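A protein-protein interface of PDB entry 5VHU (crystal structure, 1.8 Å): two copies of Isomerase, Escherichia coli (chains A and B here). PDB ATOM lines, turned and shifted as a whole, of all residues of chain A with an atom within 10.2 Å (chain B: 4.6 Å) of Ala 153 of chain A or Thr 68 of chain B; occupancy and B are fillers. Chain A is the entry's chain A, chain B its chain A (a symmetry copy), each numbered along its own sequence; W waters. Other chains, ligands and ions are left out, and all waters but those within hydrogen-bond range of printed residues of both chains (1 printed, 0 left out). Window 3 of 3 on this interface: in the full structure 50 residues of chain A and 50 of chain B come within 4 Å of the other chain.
Water W1 bridges the backbone carbonyl oxygen of Pro 154 of chain A (2.7 Å) and the side-chain hydroxyl of Thr 64 of chain B (2.7 Å).
Of the printed residues of chain B, Phe 13 of chain A touches Leu 170. Of the printed residues of chain B, Lys 53 of chain A touches Thr 64. Val 143 of chain A touches none of the printed residues of chain B. Lys 144 of chain A touches none of the printed residues of chain B. Of the printed residues of chain B, Leu 152 of chain A touches Phe 183. Printed residues of chain A within 4 Å of Thr 64 of chain B: Lys 53. No residue of chain A comes within 4 Å of Ser 67 of chain B. Thr 68 of chain B touches just one residue of chain A: Ala 153. Gly 69 of chain B touches none of the printed residues of chain A. No residue of chain A comes within 4 Å of Ala 169 of chain B. Of the printed residues of chain A, Leu 170 of chain B touches Phe 13, Ala 147 and Asp 148. The nearest residue of chain B that does not touch Ala 153 of chain A is Leu 170 of chain B (4.1 Å).
The side-chain hydroxyl of Thr 68 of chain B is in hydrogen-bond range of the backbone carbonyl oxygen of Phe 65 of chain B (3.2 Å). The backbone carbonyl oxygen of Ala 153 of chain A lies within hydrogen-bond range of the side-chain hydroxyl of Ser 155 of chain A (2.7 Å). The backbone carbonyl oxygen of Thr 68 of chain B sits at hydrogen-bond distance from the side-chain hydroxyl of Ser 173 of chain B (2.8 Å). N of Ala 147 of chain A is in hydrogen-bond range of OG of Ser 155 of chain A, 2.9 Å away. N of Ala 147 of chain A is in hydrogen-bond range of SG of Cys 156 of chain A (3.6 Å). The side-chain carboxylate of Asp 148 of chain A sits at hydrogen-bond distance from the backbone NH of Ala 153 of chain A (3.1 Å).
No position is printed for both chains.
CE2 of Phe 13 of chain A touches C of Leu 170 of chain B, 3.6 Å away. Thr 64 of chain B touches Lys 53 of chain A. CD1 of Leu 170 of chain B touches CB of Ala 147 of chain A (3.7 Å). N of Asp 148 of chain A touches CD1 of Leu 170 of chain B, 3.9 Å away. Leu 152 of chain A touches Phe 183 of chain B. CB of Ala 153 of chain A touches CG2 of Thr 68 of chain B (3.9 Å).
Of the 12 printed residues of chain B, 4 touch a printed residue of chain A. Printed residues of chain B that touch a printed residue of chain A: Thr 64, Thr 68, Leu 170 and Phe 183. Hydrophobic or aromatic side chains of chain B within 4 Å of the printed part of chain A: Leu 170 and Phe 183. Of the 24 printed residues of chain A, 6 touch a printed residue of chain B. Among the printed residues, no Asp or Glu carboxylate lies within 4 Å of a Lys or Arg side-chain nitrogen of the other chain.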
ATOM      1  N   PHE A  13       7.669  -0.163  -0.457  1.00  0.00           N
ATOM      2  CA  PHE A  13       8.893   0.646  -0.434  1.00  0.00           C
ATOM      3  C   PHE A  13       8.598   2.025  -1.054  1.00  0.00           C
ATOM      4  O   PHE A  13       9.170   3.042  -0.623  1.00  0.00           O
ATOM      5  CB  PHE A  13      10.032  -0.076  -1.168  1.00  0.00           C
ATOM      6  CG  PHE A  13      10.491  -1.325  -0.474  1.00  0.00           C
ATOM      7  CD1 PHE A  13      11.020  -1.263   0.809  1.00  0.00           C
ATOM      8  CD2 PHE A  13      10.402  -2.544  -1.117  1.00  0.00           C
ATOM      9  CE1 PHE A  13      11.476  -2.443   1.452  1.00  0.00           C
ATOM     10  CE2 PHE A  13      10.874  -3.729  -0.498  1.00  0.00           C
ATOM     11  CZ  PHE A  13      11.379  -3.659   0.805  1.00  0.00           C
ATOM     12  N   ASN A  16       6.876   4.185   1.417  1.00  0.00           N
ATOM     13  CA  ASN A  16       7.804   4.721   2.437  1.00  0.00           C
ATOM     14  C   ASN A  16       8.512   5.995   1.929  1.00  0.00           C
ATOM     15  O   ASN A  16       8.699   6.979   2.694  1.00  0.00           O
ATOM     16  CB  ASN A  16       8.878   3.734   2.882  1.00  0.00           C
ATOM     17  CG  ASN A  16       8.327   2.641   3.794  1.00  0.00           C
ATOM     18  OD1 ASN A  16       7.227   2.758   4.300  1.00  0.00           O
ATOM     19  ND2 ASN A  16       9.093   1.601   4.012  1.00  0.00           N
ATOM     20  N   GLU A  17       8.929   5.956   0.656  1.00  0.00           N
ATOM     21  CA  GLU A  17       9.520   7.196   0.021  1.00  0.00           C
ATOM     22  C   GLU A  17       8.516   8.354  -0.088  1.00  0.00           C
ATOM     23  O   GLU A  17       8.817   9.489   0.286  1.00  0.00           O
ATOM     24  CB  GLU A  17      10.161   6.895  -1.343  1.00  0.00           C
ATOM     25  CG  GLU A  17      11.336   5.948  -1.144  1.00  0.00           C
ATOM     26  CD  GLU A  17      12.340   5.987  -2.283  1.00  0.00           C
ATOM     27  OE1 GLU A  17      12.282   6.893  -3.150  1.00  0.00           O
ATOM     28  OE2 GLU A  17      13.197   5.105  -2.292  1.00  0.00           O
ATOM     29  N   GLY A  52      28.993   9.416  -2.630  1.00  0.00           N
ATOM     30  CA  GLY A  52      27.977   8.353  -2.455  1.00  0.00           C
ATOM     31  C   GLY A  52      26.660   8.727  -3.103  1.00  0.00           C
ATOM     32  O   GLY A  52      26.646   9.416  -4.128  1.00  0.00           O
ATOM     33  N   LYS A  53      25.540   8.258  -2.512  1.00  0.00           N
ATOM     34  CA  LYS A  53      24.221   8.457  -3.173  1.00  0.00           C
ATOM     35  C   LYS A  53      23.836   9.919  -3.235  1.00  0.00           C
ATOM     36  O   LYS A  53      23.321  10.365  -4.267  1.00  0.00           O
ATOM     37  CB  LYS A  53      23.121   7.668  -2.469  1.00  0.00           C
ATOM     38  CG  LYS A  53      23.356   6.166  -2.422  1.00  0.00           C
ATOM     39  CD  LYS A  53      23.831   5.521  -3.706  1.00  0.00           C
ATOM     40  CE  LYS A  53      24.067   4.016  -3.462  1.00  0.00           C
ATOM     41  NZ  LYS A  53      25.447   3.901  -2.823  1.00  0.00           N
ATOM     42  N   SER A  54      24.173  10.675  -2.183  1.00  0.00           N
ATOM     43  CA  SER A  54      23.968  12.143  -2.153  1.00  0.00           C
ATOM     44  C   SER A  54      24.693  12.804  -3.291  1.00  0.00           C
ATOM     45  O   SER A  54      24.197  13.795  -3.843  1.00  0.00           O
ATOM     46  CB  SER A  54      24.626  12.760  -0.912  1.00  0.00           C
ATOM     47  OG  SER A  54      23.902  12.476   0.182  1.00  0.00           O
ATOM     48  N   ASN A  99      23.521  13.535   4.117  1.00  0.00           N
ATOM     49  CA  ASN A  99      22.309  13.341   4.910  1.00  0.00           C
ATOM     50  C   ASN A  99      22.659  13.407   6.411  1.00  0.00           C
ATOM     51  O   ASN A  99      22.018  14.143   7.161  1.00  0.00           O
ATOM     52  CB  ASN A  99      21.672  12.004   4.578  1.00  0.00           C
ATOM     53  CG  ASN A  99      20.432  11.742   5.403  1.00  0.00           C
ATOM     54  OD1 ASN A  99      20.361  10.727   6.099  1.00  0.00           O
ATOM     55  ND2 ASN A  99      19.477  12.627   5.341  1.00  0.00           N
ATOM     56  N   VAL A 143      14.825  13.435   7.717  1.00  0.00           N
ATOM     57  CA  VAL A 143      14.414  12.182   7.122  1.00  0.00           C
ATOM     58  C   VAL A 143      14.432  11.219   8.316  1.00  0.00           C
ATOM     59  O   VAL A 143      15.532  10.942   8.875  1.00  0.00           O
ATOM     60  CB  VAL A 143      15.449  11.696   6.051  1.00  0.00           C
ATOM     61  CG1 VAL A 143      15.131  10.248   5.583  1.00  0.00           C
ATOM     62  CG2 VAL A 143      15.584  12.689   4.874  1.00  0.00           C
ATOM     63  N   LYS A 144      13.264  10.727   8.713  1.00  0.00           N
ATOM     64  CA  LYS A 144      13.141   9.802   9.897  1.00  0.00           C
ATOM     65  C   LYS A 144      13.803   8.436   9.728  1.00  0.00           C
ATOM     66  O   LYS A 144      14.450   7.921  10.672  1.00  0.00           O
ATOM     67  CB  LYS A 144      11.680   9.577  10.307  1.00  0.00           C
ATOM     68  CG  LYS A 144      11.003  10.829  10.839  1.00  0.00           C
ATOM     69  CD  LYS A 144       9.549  10.554  11.230  1.00  0.00           C
ATOM     70  CE  LYS A 144       8.841  11.805  11.736  1.00  0.00           C
ATOM     71  NZ  LYS A 144       9.530  12.393  12.929  1.00  0.00           N
ATOM     72  N   SER A 145      13.632   7.829   8.556  1.00  0.00           N
ATOM     73  CA  SER A 145      14.057   6.440   8.336  1.00  0.00           C
ATOM     74  C   SER A 145      14.287   6.231   6.844  1.00  0.00           C
ATOM     75  O   SER A 145      13.567   6.829   6.046  1.00  0.00           O
ATOM     76  CB  SER A 145      12.917   5.496   8.728  1.00  0.00           C
ATOM     77  OG  SER A 145      13.400   4.173   8.748  1.00  0.00           O
ATOM     78  N   GLU A 146      15.247   5.385   6.467  1.00  0.00           N
ATOM     79  CA  GLU A 146      15.329   4.889   5.048  1.00  0.00           C
ATOM     80  C   GLU A 146      14.256   3.826   4.782  1.00  0.00           C
ATOM     81  O   GLU A 146      13.633   3.341   5.750  1.00  0.00           O
ATOM     82  CB  GLU A 146      16.739   4.372   4.727  1.00  0.00           C
ATOM     83  CG  GLU A 146      17.843   5.396   4.956  1.00  0.00           C
ATOM     84  CD  GLU A 146      17.810   6.581   3.988  1.00  0.00           C
ATOM     85  OE1 GLU A 146      16.867   6.738   3.151  1.00  0.00           O
ATOM     86  OE2 GLU A 146      18.771   7.374   4.053  1.00  0.00           O
ATOM     87  N   ALA A 147      13.992   3.503   3.500  1.00  0.00           N
ATOM     88  CA  ALA A 147      12.849   2.662   3.140  1.00  0.00           C
ATOM     89  C   ALA A 147      13.037   1.176   3.441  1.00  0.00           C
ATOM     90  O   ALA A 147      12.022   0.437   3.519  1.00  0.00           O
ATOM     91  CB  ALA A 147      12.424   2.892   1.665  1.00  0.00           C
ATOM     92  N   ASP A 148      14.288   0.717   3.612  1.00  0.00           N
ATOM     93  CA  ASP A 148      14.544  -0.753   3.834  1.00  0.00           C
ATOM     94  C   ASP A 148      14.288  -1.142   5.309  1.00  0.00           C
ATOM     95  O   ASP A 148      14.328  -0.284   6.170  1.00  0.00           O
ATOM     96  CB  ASP A 148      15.975  -1.184   3.425  1.00  0.00           C
ATOM     97  CG  ASP A 148      17.073  -0.336   4.118  1.00  0.00           C
ATOM     98  OD1 ASP A 148      16.968   0.917   4.055  1.00  0.00           O
ATOM     99  OD2 ASP A 148      18.016  -0.893   4.765  1.00  0.00           O
ATOM    100  N   ASN A 149      14.115  -2.434   5.600  1.00  0.00           N
ATOM    101  CA  ASN A 149      13.829  -2.860   6.991  1.00  0.00           C
ATOM    102  C   ASN A 149      14.880  -2.396   8.024  1.00  0.00           C
ATOM    103  O   ASN A 149      14.527  -1.950   9.114  1.00  0.00           O
ATOM    104  CB  ASN A 149      13.616  -4.377   7.057  1.00  0.00           C
ATOM    105  CG  ASN A 149      13.634  -4.912   8.495  1.00  0.00           C
ATOM    106  OD1 ASN A 149      12.776  -4.555   9.307  1.00  0.00           O
ATOM    107  ND2 ASN A 149      14.658  -5.709   8.833  1.00  0.00           N
ATOM    108  N   LEU A 150      16.161  -2.465   7.663  1.00  0.00           N
ATOM    109  CA  LEU A 150      17.221  -2.027   8.578  1.00  0.00           C
ATOM    110  C   LEU A 150      17.560  -0.540   8.516  1.00  0.00           C
ATOM    111  O   LEU A 150      18.411  -0.044   9.310  1.00  0.00           O
ATOM    112  CB  LEU A 150      18.479  -2.855   8.361  1.00  0.00           C
ATOM    113  CG  LEU A 150      18.363  -4.328   8.826  1.00  0.00           C
ATOM    114  CD1 LEU A 150      19.703  -5.019   8.589  1.00  0.00           C
ATOM    115  CD2 LEU A 150      17.855  -4.558  10.270  1.00  0.00           C
ATOM    116  N   GLY A 151      16.944   0.166   7.561  1.00  0.00           N
ATOM    117  CA  GLY A 151      17.108   1.642   7.485  1.00  0.00           C
ATOM    118  C   GLY A 151      18.518   2.024   7.048  1.00  0.00           C
ATOM    119  O   GLY A 151      19.011   3.117   7.407  1.00  0.00           O
ATOM    120  N   LEU A 152      19.156   1.157   6.253  1.00  0.00           N
ATOM    121  CA  LEU A 152      20.551   1.379   5.854  1.00  0.00           C
ATOM    122  C   LEU A 152      20.780   2.000   4.472  1.00  0.00           C
ATOM    123  O   LEU A 152      21.823   2.637   4.255  1.00  0.00           O
ATOM    124  CB  LEU A 152      21.336   0.070   5.913  1.00  0.00           C
ATOM    125  CG  LEU A 152      21.531  -0.527   7.333  1.00  0.00           C
ATOM    126  CD1 LEU A 152      22.172  -1.894   7.198  1.00  0.00           C
ATOM    127  CD2 LEU A 152      22.338   0.424   8.235  1.00  0.00           C
ATOM    128  N   ALA A 153      19.855   1.774   3.546  1.00  0.00           N
ATOM    129  CA  ALA A 153      20.098   2.142   2.133  1.00  0.00           C
ATOM    130  C   ALA A 153      19.466   3.517   1.830  1.00  0.00           C
ATOM    131  O   ALA A 153      18.235   3.670   2.002  1.00  0.00           O
ATOM    132  CB  ALA A 153      19.524   1.076   1.204  1.00  0.00           C
ATOM    133  N   PRO A 154      20.277   4.525   1.374  1.00  0.00           N
ATOM    134  CA  PRO A 154      19.680   5.818   0.996  1.00  0.00           C
ATOM    135  C   PRO A 154      18.595   5.630  -0.063  1.00  0.00           C
ATOM    136  O   PRO A 154      18.843   5.013  -1.131  1.00  0.00           O
ATOM    137  CB  PRO A 154      20.879   6.573   0.383  1.00  0.00           C
ATOM    138  CG  PRO A 154      22.045   6.073   1.177  1.00  0.00           C
ATOM    139  CD  PRO A 154      21.755   4.618   1.491  1.00  0.00           C
ATOM    140  N   SER A 155      17.383   6.080   0.257  1.00  0.00           N
ATOM    141  CA  SER A 155      16.203   5.785  -0.570  1.00  0.00           C
ATOM    142  C   SER A 155      15.229   6.923  -0.225  1.00  0.00           C
ATOM    143  O   SER A 155      15.094   7.879  -1.009  1.00  0.00           O
ATOM    144  CB  SER A 155      15.631   4.370  -0.232  1.00  0.00           C
ATOM    145  OG  SER A 155      15.684   4.208   1.196  1.00  0.00           O
ATOM    146  N   CYS A 156      14.652   6.915   0.988  1.00  0.00           N
ATOM    147  CA  CYS A 156      13.927   8.105   1.445  1.00  0.00           C
ATOM    148  C   CYS A 156      14.810   9.368   1.416  1.00  0.00           C
ATOM    149  O   CYS A 156      14.368  10.385   0.888  1.00  0.00           O
ATOM    150  CB  CYS A 156      13.399   7.903   2.852  1.00  0.00           C
ATOM    151  SG  CYS A 156      12.217   6.547   2.925  1.00  0.00           S
ATOM    152  N   SER A 157      16.047   9.305   1.940  1.00  0.00           N
ATOM    153  CA  SER A 157      16.857  10.526   2.014  1.00  0.00           C
ATOM    154  C   SER A 157      17.255  11.071   0.622  1.00  0.00           C
ATOM    155  O   SER A 157      17.108  12.277   0.361  1.00  0.00           O
ATOM    156  CB  SER A 157      18.106  10.324   2.864  1.00  0.00           C
ATOM    157  OG  SER A 157      18.891   9.294   2.314  1.00  0.00           O
ATOM    158  N   SER A 158      17.761  10.200  -0.266  1.00  0.00           N
ATOM    159  CA  SER A 158      18.141  10.675  -1.614  1.00  0.00           C
ATOM    160  C   SER A 158      16.923  11.193  -2.382  1.00  0.00           C
ATOM    161  O   SER A 158      17.057  12.197  -3.138  1.00  0.00           O
ATOM    162  CB  SER A 158      18.917   9.552  -2.380  1.00  0.00           C
ATOM    163  OG  SER A 158      18.265   8.292  -2.149  1.00  0.00           O
ATOM    164  N   THR A 159      15.757  10.546  -2.242  1.00  0.00           N
ATOM    165  CA  THR A 159      14.575  11.035  -2.949  1.00  0.00           C
ATOM    166  C   THR A 159      14.094  12.381  -2.405  1.00  0.00           C
ATOM    167  O   THR A 159      13.730  13.242  -3.171  1.00  0.00           O
ATOM    168  CB  THR A 159      13.455   9.981  -2.917  1.00  0.00           C
ATOM    169  OG1 THR A 159      13.911   8.874  -3.706  1.00  0.00           O
ATOM    170  CG2 THR A 159      12.118  10.497  -3.517  1.00  0.00           C
ATOM    171  N   THR B  64      22.525   1.751  -6.155  1.00  0.00           N
ATOM    172  CA  THR B  64      21.589   1.235  -5.168  1.00  0.00           C
ATOM    173  C   THR B  64      21.393  -0.283  -5.325  1.00  0.00           C
ATOM    174  O   THR B  64      21.431  -1.045  -4.315  1.00  0.00           O
ATOM    175  CB  THR B  64      20.288   2.046  -5.213  1.00  0.00           C
ATOM    176  OG1 THR B  64      20.598   3.324  -4.591  1.00  0.00           O
ATOM    177  CG2 THR B  64      19.194   1.375  -4.319  1.00  0.00           C
ATOM    178  N   PHE B  65      21.231  -0.737  -6.576  1.00  0.00           N
ATOM    179  CA  PHE B  65      21.171  -2.191  -6.808  1.00  0.00           C
ATOM    180  C   PHE B  65      22.393  -2.885  -6.228  1.00  0.00           C
ATOM    181  O   PHE B  65      22.237  -3.877  -5.473  1.00  0.00           O
ATOM    182  CB  PHE B  65      21.113  -2.527  -8.332  1.00  0.00           C
ATOM    183  CG  PHE B  65      19.709  -2.596  -8.891  1.00  0.00           C
ATOM    184  CD1 PHE B  65      18.775  -1.582  -8.700  1.00  0.00           C
ATOM    185  CD2 PHE B  65      19.364  -3.705  -9.680  1.00  0.00           C
ATOM    186  CE1 PHE B  65      17.452  -1.655  -9.257  1.00  0.00           C
ATOM    187  CE2 PHE B  65      18.065  -3.802 -10.255  1.00  0.00           C
ATOM    188  CZ  PHE B  65      17.104  -2.783 -10.018  1.00  0.00           C
ATOM    189  N   ALA B  66      23.598  -2.431  -6.604  1.00  0.00           N
ATOM    190  CA  ALA B  66      24.850  -3.057  -6.157  1.00  0.00           C
ATOM    191  C   ALA B  66      25.018  -3.064  -4.635  1.00  0.00           C
ATOM    192  O   ALA B  66      25.395  -4.106  -4.060  1.00  0.00           O
ATOM    193  CB  ALA B  66      26.077  -2.340  -6.788  1.00  0.00           C
ATOM    194  N   SER B  67      24.682  -1.949  -4.011  1.00  0.00           N
ATOM    195  CA  SER B  67      24.922  -1.760  -2.567  1.00  0.00           C
ATOM    196  C   SER B  67      23.962  -2.623  -1.760  1.00  0.00           C
ATOM    197  O   SER B  67      24.196  -2.856  -0.557  1.00  0.00           O
ATOM    198  CB  SER B  67      24.758  -0.305  -2.172  1.00  0.00           C
ATOM    199  OG  SER B  67      23.429   0.097  -2.370  1.00  0.00           O
ATOM    200  N   THR B  68      22.890  -3.078  -2.412  1.00  0.00           N
ATOM    201  CA  THR B  68      21.865  -3.923  -1.773  1.00  0.00           C
ATOM    202  C   THR B  68      21.828  -5.344  -2.286  1.00  0.00           C
ATOM    203  O   THR B  68      20.865  -6.078  -1.983  1.00  0.00           O
ATOM    204  CB  THR B  68      20.452  -3.291  -1.860  1.00  0.00           C
ATOM    205  OG1 THR B  68      20.035  -3.204  -3.234  1.00  0.00           O
ATOM    206  CG2 THR B  68      20.440  -1.859  -1.186  1.00  0.00           C
ATOM    207  N   GLY B  69      22.886  -5.759  -2.996  1.00  0.00           N
ATOM    208  CA  GLY B  69      23.145  -7.179  -3.279  1.00  0.00           C
ATOM    209  C   GLY B  69      22.830  -7.647  -4.677  1.00  0.00           C
ATOM    210  O   GLY B  69      22.860  -8.823  -4.900  1.00  0.00           O
ATOM    211  N   THR B  70      22.534  -6.730  -5.610  1.00  0.00           N
ATOM    212  CA  THR B  70      22.296  -7.105  -7.010  1.00  0.00           C
ATOM    213  C   THR B  70      23.416  -6.440  -7.859  1.00  0.00           C
ATOM    214  O   THR B  70      23.327  -5.211  -8.113  1.00  0.00           O
ATOM    215  CB  THR B  70      20.918  -6.605  -7.481  1.00  0.00           C
ATOM    216  OG1 THR B  70      19.880  -7.226  -6.687  1.00  0.00           O
ATOM    217  CG2 THR B  70      20.689  -6.964  -8.974  1.00  0.00           C
ATOM    218  N   ALA B 169      14.930  -2.428  -6.375  1.00  0.00           N
ATOM    219  CA  ALA B 169      16.175  -2.818  -5.704  1.00  0.00           C
ATOM    220  C   ALA B 169      15.901  -3.398  -4.310  1.00  0.00           C
ATOM    221  O   ALA B 169      16.439  -4.462  -3.955  1.00  0.00           O
ATOM    222  CB  ALA B 169      17.122  -1.588  -5.605  1.00  0.00           C
ATOM    223  N   LEU B 170      15.085  -2.696  -3.519  1.00  0.00           N
ATOM    224  CA  LEU B 170      14.855  -3.122  -2.127  1.00  0.00           C
ATOM    225  C   LEU B 170      14.045  -4.415  -2.075  1.00  0.00           C
ATOM    226  O   LEU B 170      14.268  -5.266  -1.191  1.00  0.00           O
ATOM    227  CB  LEU B 170      14.191  -2.017  -1.292  1.00  0.00           C
ATOM    228  CG  LEU B 170      15.078  -0.759  -1.057  1.00  0.00           C
ATOM    229  CD1 LEU B 170      14.338   0.330  -0.251  1.00  0.00           C
ATOM    230  CD2 LEU B 170      16.480  -1.048  -0.482  1.00  0.00           C
ATOM    231  N   SER B 173      16.447  -7.182  -2.896  1.00  0.00           N
ATOM    232  CA  SER B 173      17.350  -7.332  -1.732  1.00  0.00           C
ATOM    233  C   SER B 173      16.667  -8.174  -0.622  1.00  0.00           C
ATOM    234  O   SER B 173      17.258  -9.149  -0.117  1.00  0.00           O
ATOM    235  CB  SER B 173      17.730  -5.960  -1.172  1.00  0.00           C
ATOM    236  OG  SER B 173      18.753  -6.059  -0.178  1.00  0.00           O
ATOM    237  N   PHE B 178      19.410 -10.508   1.717  1.00  0.00           N
ATOM    238  CA  PHE B 178      20.565  -9.667   1.922  1.00  0.00           C
ATOM    239  C   PHE B 178      20.650  -9.215   3.391  1.00  0.00           C
ATOM    240  O   PHE B 178      19.637  -8.826   3.979  1.00  0.00           O
ATOM    241  CB  PHE B 178      20.439  -8.444   0.976  1.00  0.00           C
ATOM    242  CG  PHE B 178      21.661  -7.585   0.935  1.00  0.00           C
ATOM    243  CD1 PHE B 178      22.794  -8.021   0.237  1.00  0.00           C
ATOM    244  CD2 PHE B 178      21.660  -6.335   1.556  1.00  0.00           C
ATOM    245  CE1 PHE B 178      23.920  -7.188   0.143  1.00  0.00           C
ATOM    246  CE2 PHE B 178      22.825  -5.519   1.510  1.00  0.00           C
ATOM    247  CZ  PHE B 178      23.916  -5.956   0.796  1.00  0.00           C
ATOM    248  N   PHE B 183      25.653  -5.698   3.829  1.00  0.00           N
ATOM    249  CA  PHE B 183      25.624  -4.216   3.667  1.00  0.00           C
ATOM    250  C   PHE B 183      26.948  -3.602   4.167  1.00  0.00           C
ATOM    251  O   PHE B 183      27.542  -2.714   3.468  1.00  0.00           O
ATOM    252  CB  PHE B 183      24.422  -3.552   4.362  1.00  0.00           C
ATOM    253  CG  PHE B 183      24.229  -2.114   3.956  1.00  0.00           C
ATOM    254  CD1 PHE B 183      23.461  -1.807   2.805  1.00  0.00           C
ATOM    255  CD2 PHE B 183      24.895  -1.089   4.630  1.00  0.00           C
ATOM    256  CE1 PHE B 183      23.296  -0.468   2.413  1.00  0.00           C
ATOM    257  CE2 PHE B 183      24.740   0.263   4.225  1.00  0.00           C
ATOM    258  CZ  PHE B 183      23.963   0.560   3.122  1.00  0.00           C
HETATM  259  O   HOH W   1      20.900   3.386  -1.871  1.00  0.00           O
